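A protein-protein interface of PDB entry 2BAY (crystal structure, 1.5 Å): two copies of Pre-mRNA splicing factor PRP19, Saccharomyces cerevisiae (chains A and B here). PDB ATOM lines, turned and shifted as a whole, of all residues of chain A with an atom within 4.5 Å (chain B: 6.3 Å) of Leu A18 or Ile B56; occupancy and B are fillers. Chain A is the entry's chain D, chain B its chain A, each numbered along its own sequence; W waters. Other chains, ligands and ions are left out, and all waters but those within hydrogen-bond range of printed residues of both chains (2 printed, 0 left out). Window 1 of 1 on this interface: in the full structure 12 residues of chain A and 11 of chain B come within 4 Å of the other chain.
Of the printed residues of chain B, Ile A25 touches Met B4 (3.1 Å) and Ile B56 (3.9 Å). Printed residues of chain A within 4 Å of Met B4: Met A4 (3.7 Å), Ile A25 (3.1 Å) and Ile A56 (3.9 Å). Of the printed residues of chain A, Pro B16 touches Met A4 (3.5 Å). Of the printed residues of chain A, Leu B18 touches Leu A18 and Ile A56. Printed residues of chain A within 4 Å of Ile B56: Met A4 (3.99 Å), Leu A18 (3.7 Å), Arg A23 (3.4 Å) and Ile A25 (3.9 Å). Printed residues of chain A within 4 Å of Val B57: Arg A23. The nearest residue of chain B that does not touch Leu A18 is Glu B55 (5.8 Å). The nearest printed residue of chain A that does not touch Ile B56 is Thr A24 (5.0 Å).
Met A4 touches its own counterpart, Met B4. Met A4 touches Ile B56, and with the chains exchanged Ile A56 touches Met B4. Leu A18 touches Val B54, but with the chains exchanged Val A54 does not touch Leu B18 (4.03 Å). Ile A25 touches Met B4, but with the chains exchanged Met A4 does not touch Ile B25 (4.4 Å).
CB of Pro B16 touches CE of Met A4, 3.5 Å away. Leu A18 touches Leu B18 (CD2 to CB, 3.8 Å). CG1 of Val B54 touches CD2 of Leu A18 (3.8 Å). Ile B56 touches Leu A18 (CG1 to CD1, 3.7 Å). CG of Arg A23 touches CG1 of Val B54 (3.8 Å). Arg A23 touches Ile B56 (O to CA, 3.4 Å). Met B4 touches Ile A25. CD1 of Ile A56 touches SD of Met B4, 3.9 Å away. Ile A56 touches Leu B18. Ile A56 touches Ile B25 (CG2 to CG1, 3.8 Å).
The guanidinium group of Arg A23 lies within hydrogen-bond range of the backbone carbonyl oxygen of Glu B55, 2.9 Å away. The backbone NH (N) of Val B57 is in hydrogen-bond range of the backbone carbonyl oxygen (O) of Arg A23, at 2.9 Å. SD of Met A4 sits close to O of Met B4, at 3.7 Å.
N of Ile B56 is in hydrogen-bond range of O of Pro B16 (3.1 Å). The backbone NH (N) of Leu B18 is in hydrogen-bond range of the backbone carbonyl oxygen (O) of Val B54 (2.8 Å). O of Val A54 sits at hydrogen-bond distance from N of Leu A18.
Hydrophobic or aromatic side chains of chain B within 4 Å of the printed part of chain A: Met B4, Pro B16, Leu B18, Ile B25, Val B54, Ile B56 and Val B57. Of the 11 printed residues of chain A, 5 touch a printed residue of chain B. Among the printed residues, 15 pairs touch across the chains. Among the printed residues, no Asp or Glu carboxylate lies within 4 Å of a Lys or Arg side-chain nitrogen of the other chain.
Water W2 bridges OE1 of Glu B55 (2.8 Å) and NH2 of Arg A23 (3.3 Å). Water W1 lies within hydrogen-bond range of O of Val B57 (2.8 Å) and N of Ile A25 (2.9 Å).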
ATOM      1  N   MET A   4      13.464  -9.872  25.437  1.00  0.00           N
ATOM      2  CA  MET A   4      12.435  -9.292  24.578  1.00  0.00           C
ATOM      3  C   MET A   4      11.268 -10.292  24.597  1.00  0.00           C
ATOM      4  O   MET A   4      11.402 -11.443  24.166  1.00  0.00           O
ATOM      5  CB  MET A   4      12.978  -9.111  23.156  1.00  0.00           C
ATOM      6  CG  MET A   4      14.380  -8.433  23.109  1.00  0.00           C
ATOM      7  SD  MET A   4      15.322  -8.496  21.518  1.00  0.00           S
ATOM      8  CE  MET A   4      14.290  -7.333  20.579  1.00  0.00           C
ATOM      9  N   VAL A  17       7.779 -11.240  15.658  1.00  0.00           N
ATOM     10  CA  VAL A  17       7.493 -10.256  14.645  1.00  0.00           C
ATOM     11  C   VAL A  17       7.478  -8.879  15.270  1.00  0.00           C
ATOM     12  O   VAL A  17       7.367  -8.740  16.489  1.00  0.00           O
ATOM     13  CB  VAL A  17       6.146 -10.510  13.959  1.00  0.00           C
ATOM     14  CG1 VAL A  17       6.136 -11.859  13.301  1.00  0.00           C
ATOM     15  CG2 VAL A  17       4.965 -10.334  14.933  1.00  0.00           C
ATOM     16  N   LEU A  18       7.592  -7.862  14.420  1.00  0.00           N
ATOM     17  CA  LEU A  18       7.593  -6.474  14.869  1.00  0.00           C
ATOM     18  C   LEU A  18       6.490  -5.694  14.164  1.00  0.00           C
ATOM     19  O   LEU A  18       6.361  -5.752  12.943  1.00  0.00           O
ATOM     20  CB  LEU A  18       8.944  -5.806  14.570  1.00  0.00           C
ATOM     21  CG  LEU A  18       9.328  -4.455  15.163  1.00  0.00           C
ATOM     22  CD1 LEU A  18       9.511  -4.489  16.654  1.00  0.00           C
ATOM     23  CD2 LEU A  18      10.665  -4.045  14.518  1.00  0.00           C
ATOM     24  N   SER A  19       5.690  -4.965  14.933  1.00  0.00           N
ATOM     25  CA  SER A  19       4.789  -4.001  14.308  1.00  0.00           C
ATOM     26  C   SER A  19       5.538  -2.693  14.069  1.00  0.00           C
ATOM     27  O   SER A  19       6.145  -2.166  14.974  1.00  0.00           O
ATOM     28  CB  SER A  19       3.584  -3.719  15.182  1.00  0.00           C
ATOM     29  OG  SER A  19       2.890  -2.596  14.638  1.00  0.00           O
ATOM     30  N   PRO A  20       5.479  -2.147  12.858  1.00  0.00           N
ATOM     31  CA  PRO A  20       6.099  -0.839  12.599  1.00  0.00           C
ATOM     32  C   PRO A  20       5.410   0.326  13.284  1.00  0.00           C
ATOM     33  O   PRO A  20       6.032   1.379  13.458  1.00  0.00           O
ATOM     34  CB  PRO A  20       5.993  -0.709  11.076  1.00  0.00           C
ATOM     35  CG  PRO A  20       4.796  -1.497  10.761  1.00  0.00           C
ATOM     36  CD  PRO A  20       4.850  -2.697  11.648  1.00  0.00           C
ATOM     37  N   ARG A  23       6.298  -0.390  17.164  1.00  0.00           N
ATOM     38  CA  ARG A  23       7.732  -0.738  17.243  1.00  0.00           C
ATOM     39  C   ARG A  23       7.953  -1.766  18.354  1.00  0.00           C
ATOM     40  O   ARG A  23       8.933  -1.702  19.102  1.00  0.00           O
ATOM     41  CB  ARG A  23       8.566   0.521  17.447  1.00  0.00           C
ATOM     42  CG  ARG A  23       8.528   1.503  16.269  1.00  0.00           C
ATOM     43  CD  ARG A  23       9.334   2.781  16.465  1.00  0.00           C
ATOM     44  NE  ARG A  23       8.917   3.582  17.609  1.00  0.00           N
ATOM     45  CZ  ARG A  23       9.508   3.657  18.788  1.00  0.00           C
ATOM     46  NH1 ARG A  23       9.012   4.476  19.691  1.00  0.00           N
ATOM     47  NH2 ARG A  23      10.579   2.929  19.127  1.00  0.00           N
ATOM     48  N   THR A  24       7.016  -2.706  18.439  1.00  0.00           N
ATOM     49  CA  THR A  24       6.933  -3.636  19.550  1.00  0.00           C
ATOM     50  C   THR A  24       6.966  -5.064  19.011  1.00  0.00           C
ATOM     51  O   THR A  24       6.464  -5.343  17.935  1.00  0.00           O
ATOM     52  CB  THR A  24       5.639  -3.351  20.366  1.00  0.00           C
ATOM     53  OG1 THR A  24       5.813  -2.131  21.100  1.00  0.00           O
ATOM     54  CG2 THR A  24       5.401  -4.400  21.409  1.00  0.00           C
ATOM     55  N   ILE A  25       7.587  -5.946  19.789  1.00  0.00           N
ATOM     56  CA  ILE A  25       7.697  -7.371  19.481  1.00  0.00           C
ATOM     57  C   ILE A  25       6.471  -8.138  19.921  1.00  0.00           C
ATOM     58  O   ILE A  25       5.935  -7.892  20.985  1.00  0.00           O
ATOM     59  CB  ILE A  25       8.923  -7.945  20.210  1.00  0.00           C
ATOM     60  CG1 ILE A  25      10.204  -7.289  19.691  1.00  0.00           C
ATOM     61  CG2 ILE A  25       8.975  -9.483  20.121  1.00  0.00           C
ATOM     62  CD1 ILE A  25      10.580  -7.643  18.267  1.00  0.00           C
ATOM     63  N   ILE A  53       3.414  -6.270   8.921  1.00  0.00           N
ATOM     64  CA  ILE A  53       4.099  -6.887  10.045  1.00  0.00           C
ATOM     65  C   ILE A  53       5.474  -7.356   9.555  1.00  0.00           C
ATOM     66  O   ILE A  53       5.567  -8.000   8.518  1.00  0.00           O
ATOM     67  CB  ILE A  53       3.265  -8.063  10.585  1.00  0.00           C
ATOM     68  CG1 ILE A  53       1.933  -7.556  11.185  1.00  0.00           C
ATOM     69  CG2 ILE A  53       4.054  -8.842  11.639  1.00  0.00           C
ATOM     70  CD1 ILE A  53       0.974  -8.687  11.553  1.00  0.00           C
ATOM     71  N   VAL A  54       6.527  -7.018  10.289  1.00  0.00           N
ATOM     72  CA  VAL A  54       7.872  -7.445   9.915  1.00  0.00           C
ATOM     73  C   VAL A  54       8.206  -8.770  10.596  1.00  0.00           C
ATOM     74  O   VAL A  54       8.306  -8.854  11.823  1.00  0.00           O
ATOM     75  CB  VAL A  54       8.925  -6.392  10.272  1.00  0.00           C
ATOM     76  CG1 VAL A  54      10.284  -6.820   9.752  1.00  0.00           C
ATOM     77  CG2 VAL A  54       8.541  -5.066   9.657  1.00  0.00           C
ATOM     78  N   ILE A  56      10.784 -11.331  11.661  1.00  0.00           N
ATOM     79  CA  ILE A  56      12.197 -11.215  11.993  1.00  0.00           C
ATOM     80  C   ILE A  56      12.901 -12.505  11.584  1.00  0.00           C
ATOM     81  O   ILE A  56      12.417 -13.612  11.833  1.00  0.00           O
ATOM     82  CB  ILE A  56      12.349 -10.912  13.495  1.00  0.00           C
ATOM     83  CG1 ILE A  56      11.786  -9.512  13.799  1.00  0.00           C
ATOM     84  CG2 ILE A  56      13.820 -11.018  13.970  1.00  0.00           C
ATOM     85  CD1 ILE A  56      11.604  -9.240  15.253  1.00  0.00           C
ATOM     86  N   MET B   4      16.549 -13.665  18.554  1.00  0.00           N
ATOM     87  CA  MET B   4      16.521 -12.257  18.982  1.00  0.00           C
ATOM     88  C   MET B   4      17.870 -11.777  19.551  1.00  0.00           C
ATOM     89  O   MET B   4      17.928 -10.853  20.353  1.00  0.00           O
ATOM     90  CB  MET B   4      15.341 -12.061  19.924  1.00  0.00           C
ATOM     91  CG  MET B   4      14.032 -12.237  19.146  1.00  0.00           C
ATOM     92  SD  MET B   4      13.314 -10.647  18.498  1.00  0.00           S
ATOM     93  CE  MET B   4      11.938 -10.371  19.613  1.00  0.00           C
ATOM     94  N   ARG B  15      20.133  -2.236  23.587  1.00  0.00           N
ATOM     95  CA  ARG B  15      19.221  -1.335  22.918  1.00  0.00           C
ATOM     96  C   ARG B  15      18.872  -1.959  21.566  1.00  0.00           C
ATOM     97  O   ARG B  15      19.508  -1.636  20.563  1.00  0.00           O
ATOM     98  CB  ARG B  15      19.863   0.035  22.724  1.00  0.00           C
ATOM     99  CG  ARG B  15      20.385   0.666  24.017  1.00  0.00           C
ATOM    100  CD  ARG B  15      20.686   2.147  23.892  1.00  0.00           C
ATOM    101  NE  ARG B  15      21.795   2.400  22.958  1.00  0.00           N
ATOM    102  CZ  ARG B  15      22.174   3.598  22.544  1.00  0.00           C
ATOM    103  NH1 ARG B  15      21.563   4.697  22.965  1.00  0.00           N
ATOM    104  NH2 ARG B  15      23.169   3.697  21.673  1.00  0.00           N
ATOM    105  N   PRO B  16      17.876  -2.841  21.516  1.00  0.00           N
ATOM    106  CA  PRO B  16      17.576  -3.568  20.278  1.00  0.00           C
ATOM    107  C   PRO B  16      16.957  -2.691  19.206  1.00  0.00           C
ATOM    108  O   PRO B  16      16.109  -1.833  19.484  1.00  0.00           O
ATOM    109  CB  PRO B  16      16.575  -4.636  20.718  1.00  0.00           C
ATOM    110  CG  PRO B  16      15.906  -4.036  21.872  1.00  0.00           C
ATOM    111  CD  PRO B  16      16.945  -3.219  22.596  1.00  0.00           C
ATOM    112  N   VAL B  17      17.415  -2.905  17.977  1.00  0.00           N
ATOM    113  CA  VAL B  17      16.855  -2.257  16.810  1.00  0.00           C
ATOM    114  C   VAL B  17      16.707  -3.262  15.690  1.00  0.00           C
ATOM    115  O   VAL B  17      17.300  -4.334  15.714  1.00  0.00           O
ATOM    116  CB  VAL B  17      17.707  -1.074  16.344  1.00  0.00           C
ATOM    117  CG1 VAL B  17      17.932  -0.094  17.455  1.00  0.00           C
ATOM    118  CG2 VAL B  17      19.047  -1.554  15.773  1.00  0.00           C
ATOM    119  N   LEU B  18      15.890  -2.924  14.701  1.00  0.00           N
ATOM    120  CA  LEU B  18      15.754  -3.766  13.530  1.00  0.00           C
ATOM    121  C   LEU B  18      16.075  -2.999  12.261  1.00  0.00           C
ATOM    122  O   LEU B  18      15.632  -1.862  12.077  1.00  0.00           O
ATOM    123  CB  LEU B  18      14.319  -4.298  13.441  1.00  0.00           C
ATOM    124  CG  LEU B  18      14.032  -5.122  12.185  1.00  0.00           C
ATOM    125  CD1 LEU B  18      13.404  -6.396  12.516  1.00  0.00           C
ATOM    126  CD2 LEU B  18      13.128  -4.339  11.175  1.00  0.00           C
ATOM    127  N   ILE B  25      17.763  -8.228  13.769  1.00  0.00           N
ATOM    128  CA  ILE B  25      17.978  -7.514  15.009  1.00  0.00           C
ATOM    129  C   ILE B  25      19.449  -7.194  15.198  1.00  0.00           C
ATOM    130  O   ILE B  25      20.311  -8.035  14.891  1.00  0.00           O
ATOM    131  CB  ILE B  25      17.503  -8.403  16.185  1.00  0.00           C
ATOM    132  CG1 ILE B  25      15.998  -8.664  16.049  1.00  0.00           C
ATOM    133  CG2 ILE B  25      17.880  -7.808  17.502  1.00  0.00           C
ATOM    134  CD1 ILE B  25      15.174  -7.475  16.321  1.00  0.00           C
ATOM    135  N   VAL B  54      14.518   0.768  12.772  1.00  0.00           N
ATOM    136  CA  VAL B  54      13.353   0.705  13.662  1.00  0.00           C
ATOM    137  C   VAL B  54      13.833   0.396  15.053  1.00  0.00           C
ATOM    138  O   VAL B  54      14.249  -0.718  15.346  1.00  0.00           O
ATOM    139  CB  VAL B  54      12.318  -0.352  13.230  1.00  0.00           C
ATOM    140  CG1 VAL B  54      11.108  -0.294  14.195  1.00  0.00           C
ATOM    141  CG2 VAL B  54      11.869  -0.152  11.789  1.00  0.00           C
ATOM    142  N   GLU B  55      13.778   1.381  15.953  1.00  0.00           N
ATOM    143  CA  GLU B  55      14.142   1.143  17.331  1.00  0.00           C
ATOM    144  C   GLU B  55      12.988   0.414  18.005  1.00  0.00           C
ATOM    145  O   GLU B  55      11.831   0.730  17.753  1.00  0.00           O
ATOM    146  CB  GLU B  55      14.457   2.448  18.051  1.00  0.00           C
ATOM    147  CG  GLU B  55      15.600   3.198  17.360  1.00  0.00           C
ATOM    148  CD  GLU B  55      16.181   4.345  18.167  1.00  0.00           C
ATOM    149  OE1 GLU B  55      15.560   4.769  19.166  1.00  0.00           O
ATOM    150  OE2 GLU B  55      17.267   4.822  17.789  1.00  0.00           O
ATOM    151  N   ILE B  56      13.307  -0.594  18.795  1.00  0.00           N
ATOM    152  CA  ILE B  56      12.327  -1.486  19.413  1.00  0.00           C
ATOM    153  C   ILE B  56      12.074  -1.036  20.836  1.00  0.00           C
ATOM    154  O   ILE B  56      13.000  -0.832  21.612  1.00  0.00           O
ATOM    155  CB  ILE B  56      12.813  -2.960  19.350  1.00  0.00           C
ATOM    156  CG1 ILE B  56      12.835  -3.420  17.895  1.00  0.00           C
ATOM    157  CG2 ILE B  56      11.913  -3.841  20.184  1.00  0.00           C
ATOM    158  CD1 ILE B  56      13.682  -4.681  17.665  1.00  0.00           C
ATOM    159  N   VAL B  57      10.808  -0.873  21.198  1.00  0.00           N
ATOM    160  CA  VAL B  57      10.483  -0.452  22.551  1.00  0.00           C
ATOM    161  C   VAL B  57      10.696  -1.642  23.499  1.00  0.00           C
ATOM    162  O   VAL B  57      10.170  -2.690  23.246  1.00  0.00           O
ATOM    163  CB  VAL B  57       9.013  -0.012  22.640  1.00  0.00           C
ATOM    164  CG1 VAL B  57       8.682   0.372  24.072  1.00  0.00           C
ATOM    165  CG2 VAL B  57       8.723   1.103  21.677  1.00  0.00           C
ATOM    166  N   PRO B  58      11.471  -1.507  24.568  1.00  0.00           N
ATOM    167  CA  PRO B  58      11.677  -2.664  25.468  1.00  0.00           C
ATOM    168  C   PRO B  58      10.398  -3.162  26.147  1.00  0.00           C
ATOM    169  O   PRO B  58       9.387  -2.455  26.209  1.00  0.00           O
ATOM    170  CB  PRO B  58      12.681  -2.157  26.516  1.00  0.00           C
ATOM    171  CG  PRO B  58      13.195  -0.882  26.039  1.00  0.00           C
ATOM    172  CD  PRO B  58      12.257  -0.334  24.992  1.00  0.00           C
HETATM  173  O   HOH W   1       9.004  -5.034  22.155  1.00  0.00           O
HETATM  174  O   HOH W   2      12.901   5.255  19.729  1.00  0.00           O
